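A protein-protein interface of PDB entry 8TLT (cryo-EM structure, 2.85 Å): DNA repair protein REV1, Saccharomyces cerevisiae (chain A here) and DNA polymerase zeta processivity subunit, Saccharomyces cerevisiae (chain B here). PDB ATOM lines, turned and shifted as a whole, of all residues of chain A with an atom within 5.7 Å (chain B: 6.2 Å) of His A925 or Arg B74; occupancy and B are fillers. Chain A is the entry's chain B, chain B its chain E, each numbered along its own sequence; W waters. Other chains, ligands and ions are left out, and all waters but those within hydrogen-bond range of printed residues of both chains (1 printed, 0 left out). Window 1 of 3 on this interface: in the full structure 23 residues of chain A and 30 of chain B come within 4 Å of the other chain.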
ATOM      1  N   ASN A 922       8.984 -14.456  -2.948  1.00  0.00           N
ATOM      2  CA  ASN A 922      10.416 -14.671  -2.747  1.00  0.00           C
ATOM      3  C   ASN A 922      10.694 -16.092  -2.249  1.00  0.00           C
ATOM      4  O   ASN A 922      11.355 -16.311  -1.233  1.00  0.00           O
ATOM      5  CB  ASN A 922      11.001 -13.622  -1.793  1.00  0.00           C
ATOM      6  N   ARG A 923      10.175 -17.061  -2.998  1.00  0.00           N
ATOM      7  CA  ARG A 923      10.387 -18.481  -2.742  1.00  0.00           C
ATOM      8  C   ARG A 923      10.852 -19.180  -4.008  1.00  0.00           C
ATOM      9  O   ARG A 923      10.415 -20.289  -4.324  1.00  0.00           O
ATOM     10  CB  ARG A 923       9.120 -19.145  -2.207  1.00  0.00           C
ATOM     11  CG  ARG A 923       8.392 -18.363  -1.130  1.00  0.00           C
ATOM     12  CD  ARG A 923       8.494 -19.053   0.216  1.00  0.00           C
ATOM     13  NE  ARG A 923       7.863 -18.270   1.272  1.00  0.00           N
ATOM     14  CZ  ARG A 923       6.585 -18.360   1.607  1.00  0.00           C
ATOM     15  NH1 ARG A 923       5.766 -19.195   0.991  1.00  0.00           N
ATOM     16  NH2 ARG A 923       6.116 -17.591   2.586  1.00  0.00           N
ATOM     17  N   VAL A 924      11.751 -18.534  -4.758  1.00  0.00           N
ATOM     18  CA  VAL A 924      12.211 -19.098  -6.020  1.00  0.00           C
ATOM     19  C   VAL A 924      12.981 -20.396  -5.815  1.00  0.00           C
ATOM     20  O   VAL A 924      13.060 -21.216  -6.738  1.00  0.00           O
ATOM     21  CB  VAL A 924      13.054 -18.064  -6.791  1.00  0.00           C
ATOM     22  CG1 VAL A 924      14.478 -18.023  -6.265  1.00  0.00           C
ATOM     23  CG2 VAL A 924      13.036 -18.368  -8.281  1.00  0.00           C
ATOM     24  N   HIS A 925      13.547 -20.615  -4.627  1.00  0.00           N
ATOM     25  CA  HIS A 925      14.208 -21.888  -4.356  1.00  0.00           C
ATOM     26  C   HIS A 925      13.204 -23.036  -4.357  1.00  0.00           C
ATOM     27  O   HIS A 925      13.503 -24.127  -4.854  1.00  0.00           O
ATOM     28  CB  HIS A 925      14.969 -21.825  -3.031  1.00  0.00           C
ATOM     29  CG  HIS A 925      14.173 -21.269  -1.891  1.00  0.00           C
ATOM     30  ND1 HIS A 925      13.784 -19.949  -1.824  1.00  0.00           N
ATOM     31  CD2 HIS A 925      13.710 -21.853  -0.761  1.00  0.00           C
ATOM     32  CE1 HIS A 925      13.107 -19.745  -0.709  1.00  0.00           C
ATOM     33  NE2 HIS A 925      13.047 -20.886  -0.045  1.00  0.00           N
ATOM     34  N   LEU A 926      12.005 -22.807  -3.818  1.00  0.00           N
ATOM     35  CA  LEU A 926      10.970 -23.836  -3.853  1.00  0.00           C
ATOM     36  C   LEU A 926      10.506 -24.108  -5.280  1.00  0.00           C
ATOM     37  O   LEU A 926      10.239 -25.261  -5.645  1.00  0.00           O
ATOM     38  CB  LEU A 926       9.794 -23.424  -2.972  1.00  0.00           C
ATOM     39  CG  LEU A 926      10.105 -23.077  -1.515  1.00  0.00           C
ATOM     40  CD1 LEU A 926       8.821 -22.925  -0.720  1.00  0.00           C
ATOM     41  CD2 LEU A 926      11.004 -24.129  -0.885  1.00  0.00           C
ATOM     42  N   VAL A 927      10.397 -23.060  -6.100  1.00  0.00           N
ATOM     43  CA  VAL A 927      10.032 -23.246  -7.502  1.00  0.00           C
ATOM     44  C   VAL A 927      11.095 -24.061  -8.223  1.00  0.00           C
ATOM     45  O   VAL A 927      10.782 -24.957  -9.017  1.00  0.00           O
ATOM     46  CB  VAL A 927       9.806 -21.883  -8.181  1.00  0.00           C
ATOM     47  CG1 VAL A 927       9.312 -22.076  -9.605  1.00  0.00           C
ATOM     48  CG2 VAL A 927       8.821 -21.051  -7.380  1.00  0.00           C
ATOM     49  N   LEU A 928      12.371 -23.765  -7.960  1.00  0.00           N
ATOM     50  CA  LEU A 928      13.449 -24.547  -8.554  1.00  0.00           C
ATOM     51  C   LEU A 928      13.406 -25.994  -8.081  1.00  0.00           C
ATOM     52  O   LEU A 928      13.671 -26.917  -8.859  1.00  0.00           O
ATOM     53  CB  LEU A 928      14.800 -23.914  -8.222  1.00  0.00           C
ATOM     54  CG  LEU A 928      16.032 -24.609  -8.799  1.00  0.00           C
ATOM     55  CD1 LEU A 928      16.028 -24.529 -10.316  1.00  0.00           C
ATOM     56  CD2 LEU A 928      17.303 -24.005  -8.230  1.00  0.00           C
ATOM     57  N   HIS A 929      13.084 -26.211  -6.804  1.00  0.00           N
ATOM     58  CA  HIS A 929      12.973 -27.571  -6.285  1.00  0.00           C
ATOM     59  C   HIS A 929      11.861 -28.340  -6.987  1.00  0.00           C
ATOM     60  O   HIS A 929      12.040 -29.506  -7.358  1.00  0.00           O
ATOM     61  CB  HIS A 929      12.728 -27.535  -4.777  1.00  0.00           C
ATOM     62  CG  HIS A 929      12.944 -28.850  -4.096  1.00  0.00           C
ATOM     63  ND1 HIS A 929      14.182 -29.267  -3.660  1.00  0.00           N
ATOM     64  CD2 HIS A 929      12.077 -29.839  -3.775  1.00  0.00           C
ATOM     65  CE1 HIS A 929      14.070 -30.458  -3.100  1.00  0.00           C
ATOM     66  NE2 HIS A 929      12.804 -30.828  -3.157  1.00  0.00           N
ATOM     67  N   LEU A 930      10.706 -27.702  -7.180  1.00  0.00           N
ATOM     68  CA  LEU A 930       9.608 -28.359  -7.886  1.00  0.00           C
ATOM     69  C   LEU A 930       9.980 -28.646  -9.336  1.00  0.00           C
ATOM     70  O   LEU A 930       9.654 -29.715  -9.870  1.00  0.00           O
ATOM     71  CB  LEU A 930       8.347 -27.498  -7.814  1.00  0.00           C
ATOM     72  CG  LEU A 930       7.570 -27.559  -6.497  1.00  0.00           C
ATOM     73  CD1 LEU A 930       6.505 -26.475  -6.448  1.00  0.00           C
ATOM     74  CD2 LEU A 930       6.951 -28.931  -6.302  1.00  0.00           C
ATOM     75  N   VAL B  72      14.261 -14.234  13.443  1.00  0.00           N
ATOM     76  CA  VAL B  72      15.147 -14.659  12.367  1.00  0.00           C
ATOM     77  C   VAL B  72      14.381 -15.617  11.468  1.00  0.00           C
ATOM     78  O   VAL B  72      13.913 -16.668  11.922  1.00  0.00           O
ATOM     79  CB  VAL B  72      16.420 -15.320  12.918  1.00  0.00           C
ATOM     80  CG1 VAL B  72      17.101 -16.151  11.845  1.00  0.00           C
ATOM     81  CG2 VAL B  72      17.362 -14.271  13.464  1.00  0.00           C
ATOM     82  N   TYR B  73      14.247 -15.259  10.193  1.00  0.00           N
ATOM     83  CA  TYR B  73      13.588 -16.116   9.220  1.00  0.00           C
ATOM     84  C   TYR B  73      14.554 -16.728   8.219  1.00  0.00           C
ATOM     85  O   TYR B  73      14.122 -17.491   7.350  1.00  0.00           O
ATOM     86  CB  TYR B  73      12.492 -15.342   8.475  1.00  0.00           C
ATOM     87  CG  TYR B  73      12.991 -14.262   7.540  1.00  0.00           C
ATOM     88  CD1 TYR B  73      13.189 -12.965   7.990  1.00  0.00           C
ATOM     89  CD2 TYR B  73      13.244 -14.535   6.203  1.00  0.00           C
ATOM     90  CE1 TYR B  73      13.635 -11.975   7.139  1.00  0.00           C
ATOM     91  CE2 TYR B  73      13.693 -13.550   5.345  1.00  0.00           C
ATOM     92  CZ  TYR B  73      13.886 -12.273   5.819  1.00  0.00           C
ATOM     93  OH  TYR B  73      14.331 -11.288   4.972  1.00  0.00           O
ATOM     94  N   ARG B  74      15.845 -16.424   8.318  1.00  0.00           N
ATOM     95  CA  ARG B  74      16.814 -16.931   7.351  1.00  0.00           C
ATOM     96  C   ARG B  74      18.206 -16.796   7.945  1.00  0.00           C
ATOM     97  O   ARG B  74      18.623 -15.689   8.297  1.00  0.00           O
ATOM     98  CB  ARG B  74      16.704 -16.169   6.034  1.00  0.00           C
ATOM     99  CG  ARG B  74      17.576 -16.712   4.932  1.00  0.00           C
ATOM    100  CD  ARG B  74      17.212 -16.095   3.596  1.00  0.00           C
ATOM    101  NE  ARG B  74      15.971 -16.641   3.062  1.00  0.00           N
ATOM    102  CZ  ARG B  74      15.493 -16.371   1.855  1.00  0.00           C
ATOM    103  NH1 ARG B  74      16.129 -15.563   1.024  1.00  0.00           N
ATOM    104  NH2 ARG B  74      14.347 -16.925   1.474  1.00  0.00           N
ATOM    105  N   PHE B  75      18.918 -17.914   8.060  1.00  0.00           N
ATOM    106  CA  PHE B  75      20.281 -17.940   8.573  1.00  0.00           C
ATOM    107  C   PHE B  75      21.195 -18.496   7.493  1.00  0.00           C
ATOM    108  O   PHE B  75      20.917 -19.558   6.927  1.00  0.00           O
ATOM    109  CB  PHE B  75      20.372 -18.785   9.845  1.00  0.00           C
ATOM    110  CG  PHE B  75      21.773 -19.156  10.232  1.00  0.00           C
ATOM    111  CD1 PHE B  75      22.617 -18.224  10.808  1.00  0.00           C
ATOM    112  CD2 PHE B  75      22.244 -20.441  10.032  1.00  0.00           C
ATOM    113  CE1 PHE B  75      23.904 -18.565  11.170  1.00  0.00           C
ATOM    114  CE2 PHE B  75      23.528 -20.787  10.391  1.00  0.00           C
ATOM    115  CZ  PHE B  75      24.359 -19.848  10.961  1.00  0.00           C
ATOM    116  N   SER B  76      22.282 -17.785   7.209  1.00  0.00           N
ATOM    117  CA  SER B  76      23.156 -18.117   6.095  1.00  0.00           C
ATOM    118  C   SER B  76      24.608 -18.155   6.548  1.00  0.00           C
ATOM    119  O   SER B  76      25.022 -17.369   7.404  1.00  0.00           O
ATOM    120  CB  SER B  76      22.994 -17.105   4.954  1.00  0.00           C
ATOM    121  OG  SER B  76      24.094 -17.157   4.066  1.00  0.00           O
ATOM    122  N   VAL B  92      22.346 -21.378   2.654  1.00  0.00           N
ATOM    123  CA  VAL B  92      21.232 -20.700   3.303  1.00  0.00           C
ATOM    124  C   VAL B  92      20.353 -21.729   3.997  1.00  0.00           C
ATOM    125  O   VAL B  92      19.988 -22.747   3.399  1.00  0.00           O
ATOM    126  CB  VAL B  92      20.409 -19.880   2.295  1.00  0.00           C
ATOM    127  CG1 VAL B  92      19.385 -19.040   3.023  1.00  0.00           C
ATOM    128  CG2 VAL B  92      21.321 -19.013   1.452  1.00  0.00           C
ATOM    129  N   LEU B  93      20.016 -21.458   5.255  1.00  0.00           N
ATOM    130  CA  LEU B  93      19.059 -22.248   6.020  1.00  0.00           C
ATOM    131  C   LEU B  93      17.815 -21.393   6.222  1.00  0.00           C
ATOM    132  O   LEU B  93      17.822 -20.461   7.032  1.00  0.00           O
ATOM    133  CB  LEU B  93      19.651 -22.681   7.357  1.00  0.00           C
ATOM    134  CG  LEU B  93      20.181 -24.110   7.448  1.00  0.00           C
ATOM    135  CD1 LEU B  93      20.407 -24.496   8.898  1.00  0.00           C
ATOM    136  CD2 LEU B  93      19.231 -25.081   6.773  1.00  0.00           C
ATOM    137  N   ASP B  94      16.753 -21.706   5.486  1.00  0.00           N
ATOM    138  CA  ASP B  94      15.525 -20.918   5.530  1.00  0.00           C
ATOM    139  C   ASP B  94      14.688 -21.363   6.723  1.00  0.00           C
ATOM    140  O   ASP B  94      14.198 -22.496   6.760  1.00  0.00           O
ATOM    141  CB  ASP B  94      14.751 -21.075   4.225  1.00  0.00           C
ATOM    142  CG  ASP B  94      13.616 -20.084   4.096  1.00  0.00           C
ATOM    143  OD1 ASP B  94      13.486 -19.207   4.972  1.00  0.00           O
ATOM    144  OD2 ASP B  94      12.849 -20.188   3.118  1.00  0.00           O
ATOM    145  N   PHE B  95      14.516 -20.471   7.698  1.00  0.00           N
ATOM    146  CA  PHE B  95      13.718 -20.747   8.882  1.00  0.00           C
ATOM    147  C   PHE B  95      12.325 -20.140   8.804  1.00  0.00           C
ATOM    148  O   PHE B  95      11.608 -20.128   9.808  1.00  0.00           O
ATOM    149  CB  PHE B  95      14.435 -20.249  10.136  1.00  0.00           C
ATOM    150  CG  PHE B  95      15.649 -21.049  10.496  1.00  0.00           C
ATOM    151  CD1 PHE B  95      15.534 -22.382  10.840  1.00  0.00           C
ATOM    152  CD2 PHE B  95      16.902 -20.468  10.495  1.00  0.00           C
ATOM    153  CE1 PHE B  95      16.648 -23.124  11.175  1.00  0.00           C
ATOM    154  CE2 PHE B  95      18.019 -21.205  10.830  1.00  0.00           C
ATOM    155  CZ  PHE B  95      17.892 -22.534  11.169  1.00  0.00           C
ATOM    156  N   SER B  96      11.933 -19.620   7.645  1.00  0.00           N
ATOM    157  CA  SER B  96      10.566 -19.163   7.461  1.00  0.00           C
ATOM    158  C   SER B  96       9.610 -20.349   7.484  1.00  0.00           C
ATOM    159  O   SER B  96       9.985 -21.483   7.167  1.00  0.00           O
ATOM    160  CB  SER B  96      10.427 -18.401   6.144  1.00  0.00           C
ATOM    161  N   VAL B 144      25.608 -14.751   8.543  1.00  0.00           N
ATOM    162  CA  VAL B 144      24.676 -13.671   8.245  1.00  0.00           C
ATOM    163  C   VAL B 144      23.263 -14.172   8.503  1.00  0.00           C
ATOM    164  O   VAL B 144      22.895 -15.263   8.053  1.00  0.00           O
ATOM    165  CB  VAL B 144      24.816 -13.175   6.794  1.00  0.00           C
ATOM    166  CG1 VAL B 144      23.770 -12.116   6.488  1.00  0.00           C
ATOM    167  CG2 VAL B 144      26.213 -12.637   6.547  1.00  0.00           C
ATOM    168  N   ILE B 145      22.478 -13.381   9.228  1.00  0.00           N
ATOM    169  CA  ILE B 145      21.090 -13.695   9.540  1.00  0.00           C
ATOM    170  C   ILE B 145      20.195 -12.611   8.959  1.00  0.00           C
ATOM    171  O   ILE B 145      20.573 -11.436   8.905  1.00  0.00           O
ATOM    172  CB  ILE B 145      20.864 -13.857  11.060  1.00  0.00           C
ATOM    173  CG1 ILE B 145      20.581 -12.505  11.725  1.00  0.00           C
ATOM    174  CG2 ILE B 145      22.014 -14.613  11.704  1.00  0.00           C
ATOM    175  CD1 ILE B 145      20.479 -12.560  13.232  1.00  0.00           C
ATOM    176  N   ASN B 146      19.027 -13.020   8.479  1.00  0.00           N
ATOM    177  CA  ASN B 146      18.027 -12.106   7.944  1.00  0.00           C
ATOM    178  C   ASN B 146      16.886 -12.028   8.948  1.00  0.00           C
ATOM    179  O   ASN B 146      16.170 -13.012   9.160  1.00  0.00           O
ATOM    180  CB  ASN B 146      17.535 -12.577   6.580  1.00  0.00           C
ATOM    181  CG  ASN B 146      18.463 -12.174   5.455  1.00  0.00           C
ATOM    182  OD1 ASN B 146      18.287 -11.128   4.836  1.00  0.00           O
ATOM    183  ND2 ASN B 146      19.464 -13.006   5.187  1.00  0.00           N
ATOM    184  N   ALA B 147      16.720 -10.866   9.564  1.00  0.00           N
ATOM    185  CA  ALA B 147      15.706 -10.654  10.582  1.00  0.00           C
ATOM    186  C   ALA B 147      14.585  -9.788  10.026  1.00  0.00           C
ATOM    187  O   ALA B 147      14.735  -9.127   8.997  1.00  0.00           O
ATOM    188  CB  ALA B 147      16.311 -10.003  11.826  1.00  0.00           C
ATOM    189  N   LEU B 199      22.135 -20.628  -8.270  1.00  0.00           N
ATOM    190  CA  LEU B 199      21.272 -21.079  -7.188  1.00  0.00           C
ATOM    191  C   LEU B 199      21.008 -22.574  -7.316  1.00  0.00           C
ATOM    192  O   LEU B 199      20.644 -23.053  -8.396  1.00  0.00           O
ATOM    193  CB  LEU B 199      19.950 -20.307  -7.192  1.00  0.00           C
ATOM    194  CG  LEU B 199      18.850 -20.824  -6.268  1.00  0.00           C
ATOM    195  CD1 LEU B 199      19.323 -20.815  -4.830  1.00  0.00           C
ATOM    196  CD2 LEU B 199      17.591 -19.991  -6.420  1.00  0.00           C
ATOM    197  N   THR B 200      21.189 -23.301  -6.216  1.00  0.00           N
ATOM    198  CA  THR B 200      20.933 -24.734  -6.158  1.00  0.00           C
ATOM    199  C   THR B 200      20.007 -25.024  -4.988  1.00  0.00           C
ATOM    200  O   THR B 200      20.255 -24.562  -3.869  1.00  0.00           O
ATOM    201  CB  THR B 200      22.235 -25.528  -6.011  1.00  0.00           C
ATOM    202  OG1 THR B 200      23.090 -25.257  -7.127  1.00  0.00           O
ATOM    203  CG2 THR B 200      21.950 -27.019  -5.951  1.00  0.00           C
ATOM    204  N   SER B 201      18.950 -25.790  -5.242  1.00  0.00           N
ATOM    205  CA  SER B 201      17.960 -26.127  -4.228  1.00  0.00           C
ATOM    206  C   SER B 201      18.261 -27.496  -3.632  1.00  0.00           C
ATOM    207  O   SER B 201      18.633 -28.429  -4.347  1.00  0.00           O
ATOM    208  CB  SER B 201      16.549 -26.114  -4.816  1.00  0.00           C
ATOM    209  N   HIS B 213      13.735 -25.090   5.194  1.00  0.00           N
ATOM    210  CA  HIS B 213      14.147 -25.160   3.802  1.00  0.00           C
ATOM    211  C   HIS B 213      15.618 -24.783   3.697  1.00  0.00           C
ATOM    212  O   HIS B 213      16.137 -24.013   4.510  1.00  0.00           O
ATOM    213  CB  HIS B 213      13.305 -24.231   2.926  1.00  0.00           C
ATOM    214  CG  HIS B 213      11.829 -24.422   3.086  1.00  0.00           C
ATOM    215  ND1 HIS B 213      11.249 -25.666   3.207  1.00  0.00           N
ATOM    216  CD2 HIS B 213      10.817 -23.526   3.151  1.00  0.00           C
ATOM    217  CE1 HIS B 213       9.942 -25.528   3.338  1.00  0.00           C
ATOM    218  NE2 HIS B 213       9.653 -24.239   3.306  1.00  0.00           N
ATOM    219  N   GLN B 214      16.293 -25.335   2.694  1.00  0.00           N
ATOM    220  CA  GLN B 214      17.723 -25.118   2.540  1.00  0.00           C
ATOM    221  C   GLN B 214      18.082 -25.041   1.064  1.00  0.00           C
ATOM    222  O   GLN B 214      17.553 -25.797   0.246  1.00  0.00           O
ATOM    223  CB  GLN B 214      18.517 -26.231   3.239  1.00  0.00           C
ATOM    224  CG  GLN B 214      19.766 -26.683   2.514  1.00  0.00           C
ATOM    225  CD  GLN B 214      20.240 -28.040   2.986  1.00  0.00           C
ATOM    226  OE1 GLN B 214      19.456 -28.839   3.492  1.00  0.00           O
ATOM    227  NE2 GLN B 214      21.528 -28.304   2.827  1.00  0.00           N
ATOM    228  N   PHE B 215      18.975 -24.112   0.732  1.00  0.00           N
ATOM    229  CA  PHE B 215      19.465 -23.949  -0.628  1.00  0.00           C
ATOM    230  C   PHE B 215      20.841 -23.302  -0.566  1.00  0.00           C
ATOM    231  O   PHE B 215      21.254 -22.773   0.468  1.00  0.00           O
ATOM    232  CB  PHE B 215      18.497 -23.127  -1.485  1.00  0.00           C
ATOM    233  CG  PHE B 215      18.220 -21.750  -0.951  1.00  0.00           C
ATOM    234  CD1 PHE B 215      17.228 -21.544  -0.008  1.00  0.00           C
ATOM    235  CD2 PHE B 215      18.935 -20.658  -1.408  1.00  0.00           C
ATOM    236  CE1 PHE B 215      16.967 -20.280   0.477  1.00  0.00           C
ATOM    237  CE2 PHE B 215      18.676 -19.392  -0.929  1.00  0.00           C
ATOM    238  CZ  PHE B 215      17.689 -19.202   0.013  1.00  0.00           C
HETATM  239  O   HOH W   1      11.406 -16.496   2.078  1.00  0.00           O
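A ring nitrogen (NE2) of His A925 lies within hydrogen-bond range of the side-chain carboxylate (OD2) of Asp B94, 3.2 Å away.
The guanidinium group (NH2) of Arg B74 is in salt-bridge range of the side-chain carboxylate (OD2) of Asp B94.
The backbone NH (N) of Asn B146 is in hydrogen-bond range of the backbone carbonyl oxygen (O) of Arg B74, 2.7 Å away.
O of Phe B215 is in hydrogen-bond range of N of Val B92 (2.8 Å).
N of Ser B96 is in hydrogen-bond range of OD1 of Asp B94, at 3.1 Å.
N of Asp B94 sits at hydrogen-bond distance from O of His B213 (2.6 Å).
Val A924 touches Leu B199 (CG1 to CD2, 3.7 Å).
CE1 of His A925 touches NH2 of Arg B74, at 3.8 Å.
Ser B201 touches His A925 (CB to O, 3.6 Å).
His A925 touches Phe B215 (CG to CD1, 3.6 Å).
O of Leu B199 touches CD2 of Leu A928, at 3.5 Å.
Ser B201 touches Leu A928 (N to CD2, 3.9 Å).
N of His A929 touches CB of Ser B201, at 3.996 Å.
His A925 touches just these residues of chain B: Arg B74, Asp B94, Ser B201 and Phe B215.
Of chain A, only His A925 comes within 4 Å of Arg B74.
Printed residues of chain B within 4 Å of Val A924: Leu B199 (3.7 Å).
Of the printed residues of chain B, Leu A928 touches Leu B199 (3.5 Å) and Ser B201 (3.9 Å).
Of the printed residues of chain B, His A929 touches Ser B201 (3.996 Å).
Of the printed residues of chain A, Leu B199 touches Val A924 and Leu A928.
Ser B96 touches none of the printed residues of chain A.
Of the 20 printed residues of chain B, 5 touch a printed residue of chain A.
Printed residues of chain B that touch a printed residue of chain A: Arg B74, Asp B94, Leu B199, Ser B201 and Phe B215.
Among the printed residues, 8 pairs touch across the chains.
Among the printed residues, no Asp or Glu carboxylate lies within 4 Å of a Lys or Arg side-chain nitrogen of the other chain.
Water W1 bridges the guanidinium group (NH2) of Arg B74 (3.0 Å) and the backbone carbonyl oxygen (O) of Asn A922 (3.3 Å).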
